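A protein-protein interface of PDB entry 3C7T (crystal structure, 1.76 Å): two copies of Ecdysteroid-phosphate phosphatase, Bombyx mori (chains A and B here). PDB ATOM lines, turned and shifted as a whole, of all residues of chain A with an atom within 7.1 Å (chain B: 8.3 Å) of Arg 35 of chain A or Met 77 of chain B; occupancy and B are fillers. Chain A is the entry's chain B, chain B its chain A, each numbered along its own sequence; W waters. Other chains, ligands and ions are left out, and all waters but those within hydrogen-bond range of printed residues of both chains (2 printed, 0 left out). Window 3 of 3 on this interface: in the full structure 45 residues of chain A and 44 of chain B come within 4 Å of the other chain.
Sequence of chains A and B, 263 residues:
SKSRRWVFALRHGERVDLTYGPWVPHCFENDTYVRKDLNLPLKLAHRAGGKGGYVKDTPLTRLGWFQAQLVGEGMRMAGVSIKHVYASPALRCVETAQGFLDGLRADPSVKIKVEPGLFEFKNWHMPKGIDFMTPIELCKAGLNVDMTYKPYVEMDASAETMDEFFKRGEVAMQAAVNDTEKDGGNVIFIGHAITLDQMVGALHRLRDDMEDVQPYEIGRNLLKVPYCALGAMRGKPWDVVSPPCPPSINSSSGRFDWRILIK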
ATOM      1  N   CYS A  27     -20.655   9.567  39.608  1.00  0.00           N
ATOM      2  CA  CYS A  27     -20.374   9.087  38.230  1.00  0.00           C
ATOM      3  C   CYS A  27     -21.287   7.961  37.760  1.00  0.00           C
ATOM      4  O   CYS A  27     -21.524   7.823  36.569  1.00  0.00           O
ATOM      5  CB  CYS A  27     -18.921   8.641  38.089  1.00  0.00           C
ATOM      6  SG  CYS A  27     -17.762  10.017  38.237  1.00  0.00           S
ATOM      7  N   THR A  32     -24.431   2.306  35.276  1.00  0.00           N
ATOM      8  CA  THR A  32     -23.601   2.751  34.166  1.00  0.00           C
ATOM      9  C   THR A  32     -22.717   3.896  34.609  1.00  0.00           C
ATOM     10  O   THR A  32     -23.184   4.952  35.041  1.00  0.00           O
ATOM     11  CB  THR A  32     -24.408   3.138  32.918  1.00  0.00           C
ATOM     12  OG1 THR A  32     -25.061   4.389  33.130  1.00  0.00           O
ATOM     13  CG2 THR A  32     -25.467   2.091  32.639  1.00  0.00           C
ATOM     14  N   TYR A  33     -21.432   3.639  34.520  1.00  0.00           N
ATOM     15  CA  TYR A  33     -20.427   4.637  34.832  1.00  0.00           C
ATOM     16  C   TYR A  33     -20.356   5.689  33.733  1.00  0.00           C
ATOM     17  O   TYR A  33     -20.352   5.377  32.530  1.00  0.00           O
ATOM     18  CB  TYR A  33     -19.088   3.938  34.982  1.00  0.00           C
ATOM     19  CG  TYR A  33     -17.913   4.859  35.067  1.00  0.00           C
ATOM     20  CD1 TYR A  33     -17.677   5.591  36.225  1.00  0.00           C
ATOM     21  CD2 TYR A  33     -17.012   4.983  33.995  1.00  0.00           C
ATOM     22  CE1 TYR A  33     -16.555   6.430  36.322  1.00  0.00           C
ATOM     23  CE2 TYR A  33     -15.891   5.827  34.092  1.00  0.00           C
ATOM     24  CZ  TYR A  33     -15.691   6.550  35.256  1.00  0.00           C
ATOM     25  OH  TYR A  33     -14.589   7.369  35.350  1.00  0.00           O
ATOM     26  N   VAL A  34     -20.288   6.948  34.147  1.00  0.00           N
ATOM     27  CA  VAL A  34     -20.100   8.041  33.209  1.00  0.00           C
ATOM     28  C   VAL A  34     -18.869   8.777  33.690  1.00  0.00           C
ATOM     29  O   VAL A  34     -18.779   9.126  34.850  1.00  0.00           O
ATOM     30  CB  VAL A  34     -21.298   9.020  33.165  1.00  0.00           C
ATOM     31  CG1 VAL A  34     -20.977  10.173  32.206  1.00  0.00           C
ATOM     32  CG2 VAL A  34     -22.603   8.305  32.765  1.00  0.00           C
ATOM     33  N   ARG A  35     -17.904   8.974  32.804  1.00  0.00           N
ATOM     34  CA  ARG A  35     -16.718   9.736  33.161  1.00  0.00           C
ATOM     35  C   ARG A  35     -17.090  11.215  33.283  1.00  0.00           C
ATOM     36  O   ARG A  35     -17.519  11.839  32.296  1.00  0.00           O
ATOM     37  CB  ARG A  35     -15.662   9.558  32.077  1.00  0.00           C
ATOM     38  CG  ARG A  35     -14.331  10.104  32.508  1.00  0.00           C
ATOM     39  CD  ARG A  35     -13.350  10.161  31.369  1.00  0.00           C
ATOM     40  NE  ARG A  35     -13.864  10.967  30.262  1.00  0.00           N
ATOM     41  CZ  ARG A  35     -13.106  11.509  29.315  1.00  0.00           C
ATOM     42  NH1 ARG A  35     -11.801  11.332  29.318  1.00  0.00           N
ATOM     43  NH2 ARG A  35     -13.669  12.213  28.344  1.00  0.00           N
ATOM     44  N   LYS A  36     -16.922  11.782  34.478  1.00  0.00           N
ATOM     45  CA  LYS A  36     -17.309  13.160  34.726  1.00  0.00           C
ATOM     46  C   LYS A  36     -16.116  14.114  34.888  1.00  0.00           C
ATOM     47  O   LYS A  36     -16.296  15.295  35.202  1.00  0.00           O
ATOM     48  CB  LYS A  36     -18.159  13.221  35.988  1.00  0.00           C
ATOM     49  CG  LYS A  36     -19.410  12.392  35.915  1.00  0.00           C
ATOM     50  CD  LYS A  36     -20.468  13.163  35.178  1.00  0.00           C
ATOM     51  CE  LYS A  36     -21.801  12.799  35.751  1.00  0.00           C
ATOM     52  NZ  LYS A  36     -22.075  11.373  35.511  1.00  0.00           N
ATOM     53  N   ASP A  37     -14.909  13.597  34.693  1.00  0.00           N
ATOM     54  CA  ASP A  37     -13.685  14.411  34.813  1.00  0.00           C
ATOM     55  C   ASP A  37     -12.597  13.740  33.980  1.00  0.00           C
ATOM     56  O   ASP A  37     -12.575  12.511  33.875  1.00  0.00           O
ATOM     57  CB  ASP A  37     -13.271  14.478  36.293  1.00  0.00           C
ATOM     58  CG  ASP A  37     -12.189  15.499  36.556  1.00  0.00           C
ATOM     59  OD1 ASP A  37     -12.515  16.658  36.836  1.00  0.00           O
ATOM     60  OD2 ASP A  37     -11.006  15.142  36.530  1.00  0.00           O
ATOM     61  N   LEU A  38     -11.691  14.533  33.401  1.00  0.00           N
ATOM     62  CA  LEU A  38     -10.715  13.987  32.477  1.00  0.00           C
ATOM     63  C   LEU A  38      -9.696  13.145  33.209  1.00  0.00           C
ATOM     64  O   LEU A  38      -9.033  12.316  32.595  1.00  0.00           O
ATOM     65  CB  LEU A  38      -9.996  15.108  31.709  1.00  0.00           C
ATOM     66  CG  LEU A  38     -10.844  15.947  30.742  1.00  0.00           C
ATOM     67  CD1 LEU A  38      -9.932  16.873  30.009  1.00  0.00           C
ATOM     68  CD2 LEU A  38     -11.552  15.035  29.720  1.00  0.00           C
ATOM     69  N   ASN A  39      -9.546  13.368  34.512  1.00  0.00           N
ATOM     70  CA  ASN A  39      -8.568  12.580  35.283  1.00  0.00           C
ATOM     71  C   ASN A  39      -9.170  11.285  35.886  1.00  0.00           C
ATOM     72  O   ASN A  39      -8.492  10.478  36.529  1.00  0.00           O
ATOM     73  CB  ASN A  39      -7.832  13.505  36.290  1.00  0.00           C
ATOM     74  CG  ASN A  39      -6.571  12.866  36.863  1.00  0.00           C
ATOM     75  OD1 ASN A  39      -5.888  12.122  36.169  1.00  0.00           O
ATOM     76  ND2 ASN A  39      -6.291  13.133  38.141  1.00  0.00           N
ATOM     77  N   LEU A  40     -10.431  11.027  35.591  1.00  0.00           N
ATOM     78  CA  LEU A  40     -11.047   9.764  35.983  1.00  0.00           C
ATOM     79  C   LEU A  40     -10.830   8.713  34.903  1.00  0.00           C
ATOM     80  O   LEU A  40     -10.577   9.075  33.739  1.00  0.00           O
ATOM     81  CB  LEU A  40     -12.547   9.969  36.201  1.00  0.00           C
ATOM     82  CG  LEU A  40     -12.862  10.682  37.520  1.00  0.00           C
ATOM     83  CD1 LEU A  40     -14.298  11.054  37.513  1.00  0.00           C
ATOM     84  CD2 LEU A  40     -12.515   9.835  38.764  1.00  0.00           C
ATOM     85  N   PRO A  41     -10.957   7.413  35.265  1.00  0.00           N
ATOM     86  CA  PRO A  41     -10.890   6.334  34.278  1.00  0.00           C
ATOM     87  C   PRO A  41     -11.875   6.507  33.124  1.00  0.00           C
ATOM     88  O   PRO A  41     -12.990   7.029  33.311  1.00  0.00           O
ATOM     89  CB  PRO A  41     -11.255   5.092  35.095  1.00  0.00           C
ATOM     90  CG  PRO A  41     -10.978   5.415  36.492  1.00  0.00           C
ATOM     91  CD  PRO A  41     -11.149   6.892  36.640  1.00  0.00           C
ATOM     92  N   LEU A  42     -11.468   6.088  31.923  1.00  0.00           N
ATOM     93  CA  LEU A  42     -12.369   6.166  30.760  1.00  0.00           C
ATOM     94  C   LEU A  42     -13.575   5.239  30.952  1.00  0.00           C
ATOM     95  O   LEU A  42     -14.701   5.564  30.598  1.00  0.00           O
ATOM     96  CB  LEU A  42     -11.613   5.712  29.515  1.00  0.00           C
ATOM     97  CG  LEU A  42     -10.583   6.688  28.955  1.00  0.00           C
ATOM     98  CD1 LEU A  42      -9.854   5.984  27.817  1.00  0.00           C
ATOM     99  CD2 LEU A  42     -11.252   7.978  28.502  1.00  0.00           C
ATOM    100  N   LYS A  43     -13.309   4.080  31.530  1.00  0.00           N
ATOM    101  CA  LYS A  43     -14.356   3.092  31.815  1.00  0.00           C
ATOM    102  C   LYS A  43     -13.922   2.277  33.018  1.00  0.00           C
ATOM    103  O   LYS A  43     -12.758   2.341  33.422  1.00  0.00           O
ATOM    104  CB  LYS A  43     -14.590   2.150  30.614  1.00  0.00           C
ATOM    105  CG  LYS A  43     -14.895   2.756  29.225  1.00  0.00           C
ATOM    106  CD  LYS A  43     -15.076   1.620  28.216  1.00  0.00           C
ATOM    107  CE  LYS A  43     -15.077   2.097  26.759  1.00  0.00           C
ATOM    108  NZ  LYS A  43     -15.338   0.953  25.832  1.00  0.00           N
ATOM    109  N   ARG A  62      -6.104   8.898  35.866  1.00  0.00           N
ATOM    110  CA  ARG A  62      -5.281   8.982  34.641  1.00  0.00           C
ATOM    111  C   ARG A  62      -3.835   9.398  34.950  1.00  0.00           C
ATOM    112  O   ARG A  62      -2.870   8.821  34.420  1.00  0.00           O
ATOM    113  CB  ARG A  62      -5.890   9.943  33.597  1.00  0.00           C
ATOM    114  CG  ARG A  62      -7.236   9.484  33.022  1.00  0.00           C
ATOM    115  CD  ARG A  62      -7.175   8.182  32.205  1.00  0.00           C
ATOM    116  NE  ARG A  62      -6.322   8.243  30.990  1.00  0.00           N
ATOM    117  CZ  ARG A  62      -6.704   8.722  29.796  1.00  0.00           C
ATOM    118  NH1 ARG A  62      -7.908   9.212  29.603  1.00  0.00           N
ATOM    119  NH2 ARG A  62      -5.861   8.709  28.764  1.00  0.00           N
ATOM    120  N   ARG A 255     -10.361  22.069  39.476  1.00  0.00           N
ATOM    121  CA  ARG A 255     -11.360  21.763  38.480  1.00  0.00           C
ATOM    122  C   ARG A 255     -12.034  23.057  38.041  1.00  0.00           C
ATOM    123  O   ARG A 255     -12.533  23.812  38.882  1.00  0.00           O
ATOM    124  CB  ARG A 255     -12.379  20.836  39.097  1.00  0.00           C
ATOM    125  CG  ARG A 255     -13.054  19.974  38.105  1.00  0.00           C
ATOM    126  CD  ARG A 255     -13.817  18.901  38.857  1.00  0.00           C
ATOM    127  NE  ARG A 255     -14.514  18.011  37.936  1.00  0.00           N
ATOM    128  CZ  ARG A 255     -15.823  18.019  37.737  1.00  0.00           C
ATOM    129  NH1 ARG A 255     -16.602  18.879  38.374  1.00  0.00           N
ATOM    130  NH2 ARG A 255     -16.347  17.145  36.900  1.00  0.00           N
ATOM    131  N   GLN B  69      -3.120  16.763  26.255  1.00  0.00           N
ATOM    132  CA  GLN B  69      -3.524  15.547  25.544  1.00  0.00           C
ATOM    133  C   GLN B  69      -4.891  15.052  25.986  1.00  0.00           C
ATOM    134  O   GLN B  69      -5.695  14.661  25.160  1.00  0.00           O
ATOM    135  CB  GLN B  69      -2.495  14.453  25.744  1.00  0.00           C
ATOM    136  CG  GLN B  69      -1.209  14.744  25.029  1.00  0.00           C
ATOM    137  CD  GLN B  69      -0.017  13.944  25.548  1.00  0.00           C
ATOM    138  OE1 GLN B  69      -0.164  12.997  26.333  1.00  0.00           O
ATOM    139  NE2 GLN B  69       1.170  14.326  25.104  1.00  0.00           N
ATOM    140  N   LEU B  70      -5.154  15.090  27.291  1.00  0.00           N
ATOM    141  CA  LEU B  70      -6.440  14.680  27.824  1.00  0.00           C
ATOM    142  C   LEU B  70      -7.590  15.517  27.284  1.00  0.00           C
ATOM    143  O   LEU B  70      -8.697  14.978  27.008  1.00  0.00           O
ATOM    144  CB  LEU B  70      -6.433  14.748  29.346  1.00  0.00           C
ATOM    145  CG  LEU B  70      -5.607  13.658  30.001  1.00  0.00           C
ATOM    146  CD1 LEU B  70      -5.575  14.000  31.504  1.00  0.00           C
ATOM    147  CD2 LEU B  70      -6.193  12.255  29.730  1.00  0.00           C
ATOM    148  N   VAL B  71      -7.348  16.821  27.138  1.00  0.00           N
ATOM    149  CA  VAL B  71      -8.346  17.691  26.520  1.00  0.00           C
ATOM    150  C   VAL B  71      -8.591  17.305  25.038  1.00  0.00           C
ATOM    151  O   VAL B  71      -9.749  17.118  24.626  1.00  0.00           O
ATOM    152  CB  VAL B  71      -8.002  19.193  26.682  1.00  0.00           C
ATOM    153  CG1 VAL B  71      -9.068  20.069  25.937  1.00  0.00           C
ATOM    154  CG2 VAL B  71      -7.895  19.575  28.174  1.00  0.00           C
ATOM    155  N   GLY B  72      -7.515  17.151  24.262  1.00  0.00           N
ATOM    156  CA  GLY B  72      -7.642  16.751  22.826  1.00  0.00           C
ATOM    157  C   GLY B  72      -8.382  15.418  22.694  1.00  0.00           C
ATOM    158  O   GLY B  72      -9.309  15.282  21.869  1.00  0.00           O
ATOM    159  N   GLU B  73      -8.009  14.453  23.539  1.00  0.00           N
ATOM    160  CA  GLU B  73      -8.645  13.118  23.596  1.00  0.00           C
ATOM    161  C   GLU B  73     -10.137  13.265  23.916  1.00  0.00           C
ATOM    162  O   GLU B  73     -10.979  12.594  23.307  1.00  0.00           O
ATOM    163  CB  GLU B  73      -7.934  12.220  24.625  1.00  0.00           C
ATOM    164  CG  GLU B  73      -8.363  10.725  24.663  1.00  0.00           C
ATOM    165  CD  GLU B  73      -7.883   9.963  25.928  1.00  0.00           C
ATOM    166  OE1 GLU B  73      -8.098  10.427  27.060  1.00  0.00           O
ATOM    167  OE2 GLU B  73      -7.313   8.858  25.796  1.00  0.00           O
ATOM    168  N   GLY B  74     -10.462  14.153  24.858  1.00  0.00           N
ATOM    169  CA  GLY B  74     -11.836  14.352  25.299  1.00  0.00           C
ATOM    170  C   GLY B  74     -12.673  14.936  24.176  1.00  0.00           C
ATOM    171  O   GLY B  74     -13.847  14.556  24.009  1.00  0.00           O
ATOM    172  N   MET B  75     -12.054  15.826  23.399  1.00  0.00           N
ATOM    173  CA  MET B  75     -12.698  16.420  22.227  1.00  0.00           C
ATOM    174  C   MET B  75     -12.972  15.327  21.183  1.00  0.00           C
ATOM    175  O   MET B  75     -14.081  15.246  20.649  1.00  0.00           O
ATOM    176  CB  MET B  75     -11.824  17.556  21.665  1.00  0.00           C
ATOM    177  CG  MET B  75     -12.649  18.643  20.950  1.00  0.00           C
ATOM    178  SD  MET B  75     -13.453  19.756  22.114  1.00  0.00           S
ATOM    179  CE  MET B  75     -12.144  20.940  22.508  1.00  0.00           C
ATOM    180  N   ARG B  76     -11.964  14.481  20.920  1.00  0.00           N
ATOM    181  CA  ARG B  76     -12.087  13.344  20.000  1.00  0.00           C
ATOM    182  C   ARG B  76     -13.208  12.396  20.445  1.00  0.00           C
ATOM    183  O   ARG B  76     -14.018  11.948  19.627  1.00  0.00           O
ATOM    184  CB  ARG B  76     -10.741  12.597  19.874  1.00  0.00           C
ATOM    185  CG  ARG B  76     -10.776  11.270  19.049  1.00  0.00           C
ATOM    186  CD  ARG B  76      -9.394  10.838  18.594  1.00  0.00           C
ATOM    187  NE  ARG B  76      -8.389  10.855  19.663  1.00  0.00           N
ATOM    188  CZ  ARG B  76      -8.081   9.827  20.461  1.00  0.00           C
ATOM    189  NH1 ARG B  76      -8.692   8.640  20.340  1.00  0.00           N
ATOM    190  NH2 ARG B  76      -7.136   9.987  21.386  1.00  0.00           N
ATOM    191  N   MET B  77     -13.275  12.097  21.741  1.00  0.00           N
ATOM    192  CA  MET B  77     -14.341  11.225  22.250  1.00  0.00           C
ATOM    193  C   MET B  77     -15.725  11.792  22.079  1.00  0.00           C
ATOM    194  O   MET B  77     -16.694  11.037  21.923  1.00  0.00           O
ATOM    195  CB  MET B  77     -14.113  10.941  23.704  1.00  0.00           C
ATOM    196  CG  MET B  77     -12.971  10.033  23.859  1.00  0.00           C
ATOM    197  SD  MET B  77     -12.404  10.021  25.530  1.00  0.00           S
ATOM    198  CE  MET B  77     -11.274   8.643  25.329  1.00  0.00           C
ATOM    199  N   ALA B  78     -15.824  13.112  22.124  1.00  0.00           N
ATOM    200  CA  ALA B  78     -17.103  13.803  21.984  1.00  0.00           C
ATOM    201  C   ALA B  78     -17.506  14.007  20.515  1.00  0.00           C
ATOM    202  O   ALA B  78     -18.545  14.599  20.227  1.00  0.00           O
ATOM    203  CB  ALA B  78     -17.049  15.123  22.714  1.00  0.00           C
ATOM    204  N   GLY B  79     -16.672  13.509  19.603  1.00  0.00           N
ATOM    205  CA  GLY B  79     -16.894  13.660  18.157  1.00  0.00           C
ATOM    206  C   GLY B  79     -16.674  15.055  17.623  1.00  0.00           C
ATOM    207  O   GLY B  79     -17.184  15.407  16.548  1.00  0.00           O
ATOM    208  N   VAL B  80     -15.926  15.876  18.357  1.00  0.00           N
ATOM    209  CA  VAL B  80     -15.708  17.248  17.931  1.00  0.00           C
ATOM    210  C   VAL B  80     -14.359  17.406  17.223  1.00  0.00           C
ATOM    211  O   VAL B  80     -13.314  17.030  17.758  1.00  0.00           O
ATOM    212  CB  VAL B  80     -15.872  18.270  19.097  1.00  0.00           C
ATOM    213  CG1 VAL B  80     -15.635  19.704  18.592  1.00  0.00           C
ATOM    214  CG2 VAL B  80     -17.265  18.154  19.717  1.00  0.00           C
ATOM    215  N   SER B  81     -14.394  17.948  16.007  1.00  0.00           N
ATOM    216  CA  SER B  81     -13.173  18.197  15.236  1.00  0.00           C
ATOM    217  C   SER B  81     -12.704  19.632  15.470  1.00  0.00           C
ATOM    218  O   SER B  81     -13.459  20.442  16.003  1.00  0.00           O
ATOM    219  CB  SER B  81     -13.441  17.979  13.745  1.00  0.00           C
ATOM    220  OG  SER B  81     -14.571  18.738  13.349  1.00  0.00           O
ATOM    221  N   GLY B 103      -3.649  14.501  21.276  1.00  0.00           N
ATOM    222  CA  GLY B 103      -4.777  13.816  21.923  1.00  0.00           C
ATOM    223  C   GLY B 103      -5.949  13.688  20.961  1.00  0.00           C
ATOM    224  O   GLY B 103      -6.628  12.631  20.895  1.00  0.00           O
ATOM    225  N   LEU B 104      -6.172  14.760  20.206  1.00  0.00           N
ATOM    226  CA  LEU B 104      -7.211  14.839  19.175  1.00  0.00           C
ATOM    227  C   LEU B 104      -6.981  13.891  17.986  1.00  0.00           C
ATOM    228  O   LEU B 104      -7.922  13.538  17.273  1.00  0.00           O
ATOM    229  CB  LEU B 104      -7.326  16.289  18.680  1.00  0.00           C
ATOM    230  CG  LEU B 104      -8.489  16.737  17.792  1.00  0.00           C
ATOM    231  CD1 LEU B 104      -9.844  16.426  18.449  1.00  0.00           C
ATOM    232  CD2 LEU B 104      -8.382  18.212  17.447  1.00  0.00           C
ATOM    233  N   PRO B 244     -17.779  20.342  25.204  1.00  0.00           N
ATOM    234  CA  PRO B 244     -18.243  18.975  24.905  1.00  0.00           C
ATOM    235  C   PRO B 244     -17.548  17.863  25.695  1.00  0.00           C
ATOM    236  O   PRO B 244     -17.963  16.700  25.610  1.00  0.00           O
ATOM    237  CB  PRO B 244     -17.926  18.820  23.419  1.00  0.00           C
ATOM    238  CG  PRO B 244     -16.763  19.764  23.195  1.00  0.00           C
ATOM    239  CD  PRO B 244     -16.989  20.920  24.097  1.00  0.00           C
ATOM    240  N   CYS B 245     -16.493  18.217  26.428  1.00  0.00           N
ATOM    241  CA  CYS B 245     -15.769  17.261  27.265  1.00  0.00           C
ATOM    242  C   CYS B 245     -15.642  17.791  28.697  1.00  0.00           C
ATOM    243  O   CYS B 245     -15.693  19.013  28.906  1.00  0.00           O
ATOM    244  CB  CYS B 245     -14.405  16.958  26.646  1.00  0.00           C
ATOM    245  SG  CYS B 245     -13.209  18.314  26.743  1.00  0.00           S
ATOM    246  N   PRO B 246     -15.470  16.889  29.690  1.00  0.00           N
ATOM    247  CA  PRO B 246     -15.463  17.315  31.110  1.00  0.00           C
ATOM    248  C   PRO B 246     -14.264  18.191  31.503  1.00  0.00           C
ATOM    249  O   PRO B 246     -13.289  18.261  30.763  1.00  0.00           O
ATOM    250  CB  PRO B 246     -15.419  15.989  31.896  1.00  0.00           C
ATOM    251  CG  PRO B 246     -15.266  14.895  30.906  1.00  0.00           C
ATOM    252  CD  PRO B 246     -15.239  15.438  29.522  1.00  0.00           C
ATOM    253  N   PRO B 247     -14.334  18.840  32.675  1.00  0.00           N
ATOM    254  CA  PRO B 247     -13.157  19.499  33.251  1.00  0.00           C
ATOM    255  C   PRO B 247     -12.227  18.451  33.859  1.00  0.00           C
ATOM    256  O   PRO B 247     -12.489  17.254  33.714  1.00  0.00           O
ATOM    257  CB  PRO B 247     -13.746  20.395  34.342  1.00  0.00           C
ATOM    258  CG  PRO B 247     -14.996  19.752  34.745  1.00  0.00           C
ATOM    259  CD  PRO B 247     -15.530  18.988  33.528  1.00  0.00           C
HETATM  260  O   HOH W   1     -15.110  13.495  26.283  1.00  0.00           O
HETATM  261  O   HOH W   2      -9.556  12.498  27.837  1.00  0.00           O
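Printed residues of chain A within 4 Å of Met 77 of chain B: Arg 35 (3.8 Å) and Leu 42 (3.2 Å).
Of the printed residues of chain B, Leu 38 of chain A touches Leu 70, Val 71, Pro 246 and Pro 247.
Printed residues of chain A within 4 Å of Pro 246 of chain B: Arg 35, Lys 36, Asp 37 and Leu 38.
Of the printed residues of chain B, Leu 42 of chain A touches Met 77.
Of the printed residues of chain A, Glu 73 of chain B touches Arg 62.
Gln 69 of chain B touches none of the printed residues of chain A.
Cys 27 of chain A touches none of the printed residues of chain B.
Of the 15 printed residues of chain A, 7 touch a printed residue of chain B.
Hydrophobic or aromatic side chains of chain A that line the printed part of chain B: Leu 38 and Leu 42.
Of the 19 printed residues of chain B, 6 touch a printed residue of chain A.
Printed residues of chain B that touch a printed residue of chain A: Leu 70, Val 71, Glu 73, Met 77, Pro 246 and Pro 247.
Hydrophobic or aromatic side chains of chain B that line the printed part of chain A: Leu 70, Val 71, Met 77, Pro 246 and Pro 247.
Among the printed residues, 13 pairs touch across the chains.
Among the printed residues, Asp or Glu carboxylates within 4 Å of a Lys or Arg side-chain nitrogen of the other chain: Arg 62 of chain A with Glu 73 of chain B.
The backbone NH (N) of Glu 73 of chain B lies close to the backbone carbonyl oxygen (O) of Gly 103 of chain B (3.5 Å).
O of Lys 36 of chain A sits at hydrogen-bond distance from NH2 of Arg 255 of chain A (2.5 Å).
The side-chain carboxylate of Asp 37 of chain A is in hydrogen-bond range of the backbone NH of Asn 39 of chain A (3.1 Å).
OD1 of Asp 37 of chain A is in salt-bridge range of NE of Arg 255 of chain A.
N of Arg 62 of chain A is in hydrogen-bond range of O of Asn 39 of chain A.
Water W2 lies within hydrogen-bond range of OE1 of Glu 73 of chain B (2.6 Å), O of Leu 70 of chain B (2.8 Å) and NH1 of Arg 35 of chain A (2.9 Å).
Water W1 lies within hydrogen-bond range of O of Gly 74 of chain B (2.8 Å) and NH2 of Arg 35 of chain A (2.8 Å).
No position is printed for both chains.
Of the 13 pairs that touch across the chains among the printed residues, none has its exchanged pair printed and touching as well.
NH2 of Arg 35 of chain A touches CD of Pro 246 of chain B, at 3.8 Å.
Lys 36 of chain A touches Pro 246 of chain B.
N of Asp 37 of chain A touches CB of Pro 246 of chain B (3.7 Å).
Leu 70 of chain B touches Leu 38 of chain A.
CD1 of Leu 38 of chain A touches CG2 of Val 71 of chain B (3.8 Å).
Pro 246 of chain B touches Leu 38 of chain A.
Leu 42 of chain A touches Met 77 of chain B.
Arg 62 of chain A touches Leu 70 of chain B (NH1 to CD2, 3.5 Å).
Arg 255 of chain A touches Pro 247 of chain B.
The side-chain carboxylate (OE1) of Glu 73 of chain B lies within salt-bridge range of the guanidinium group (NH1) of Arg 62 of chain A (2.8 Å).
The side-chain sulfur (SD) of Met 77 of chain B sits at hydrogen-bond distance from the guanidinium group (NH2) of Arg 35 of chain A, at 3.8 Å.
O of Pro 247 of chain B lies within hydrogen-bond range of N of Leu 38 of chain A (2.9 Å).
The side-chain carboxylate (OD1) of Asp 37 of chain A sits close to the backbone carbonyl oxygen (O) of Pro 247 of chain B, at 3.2 Å.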
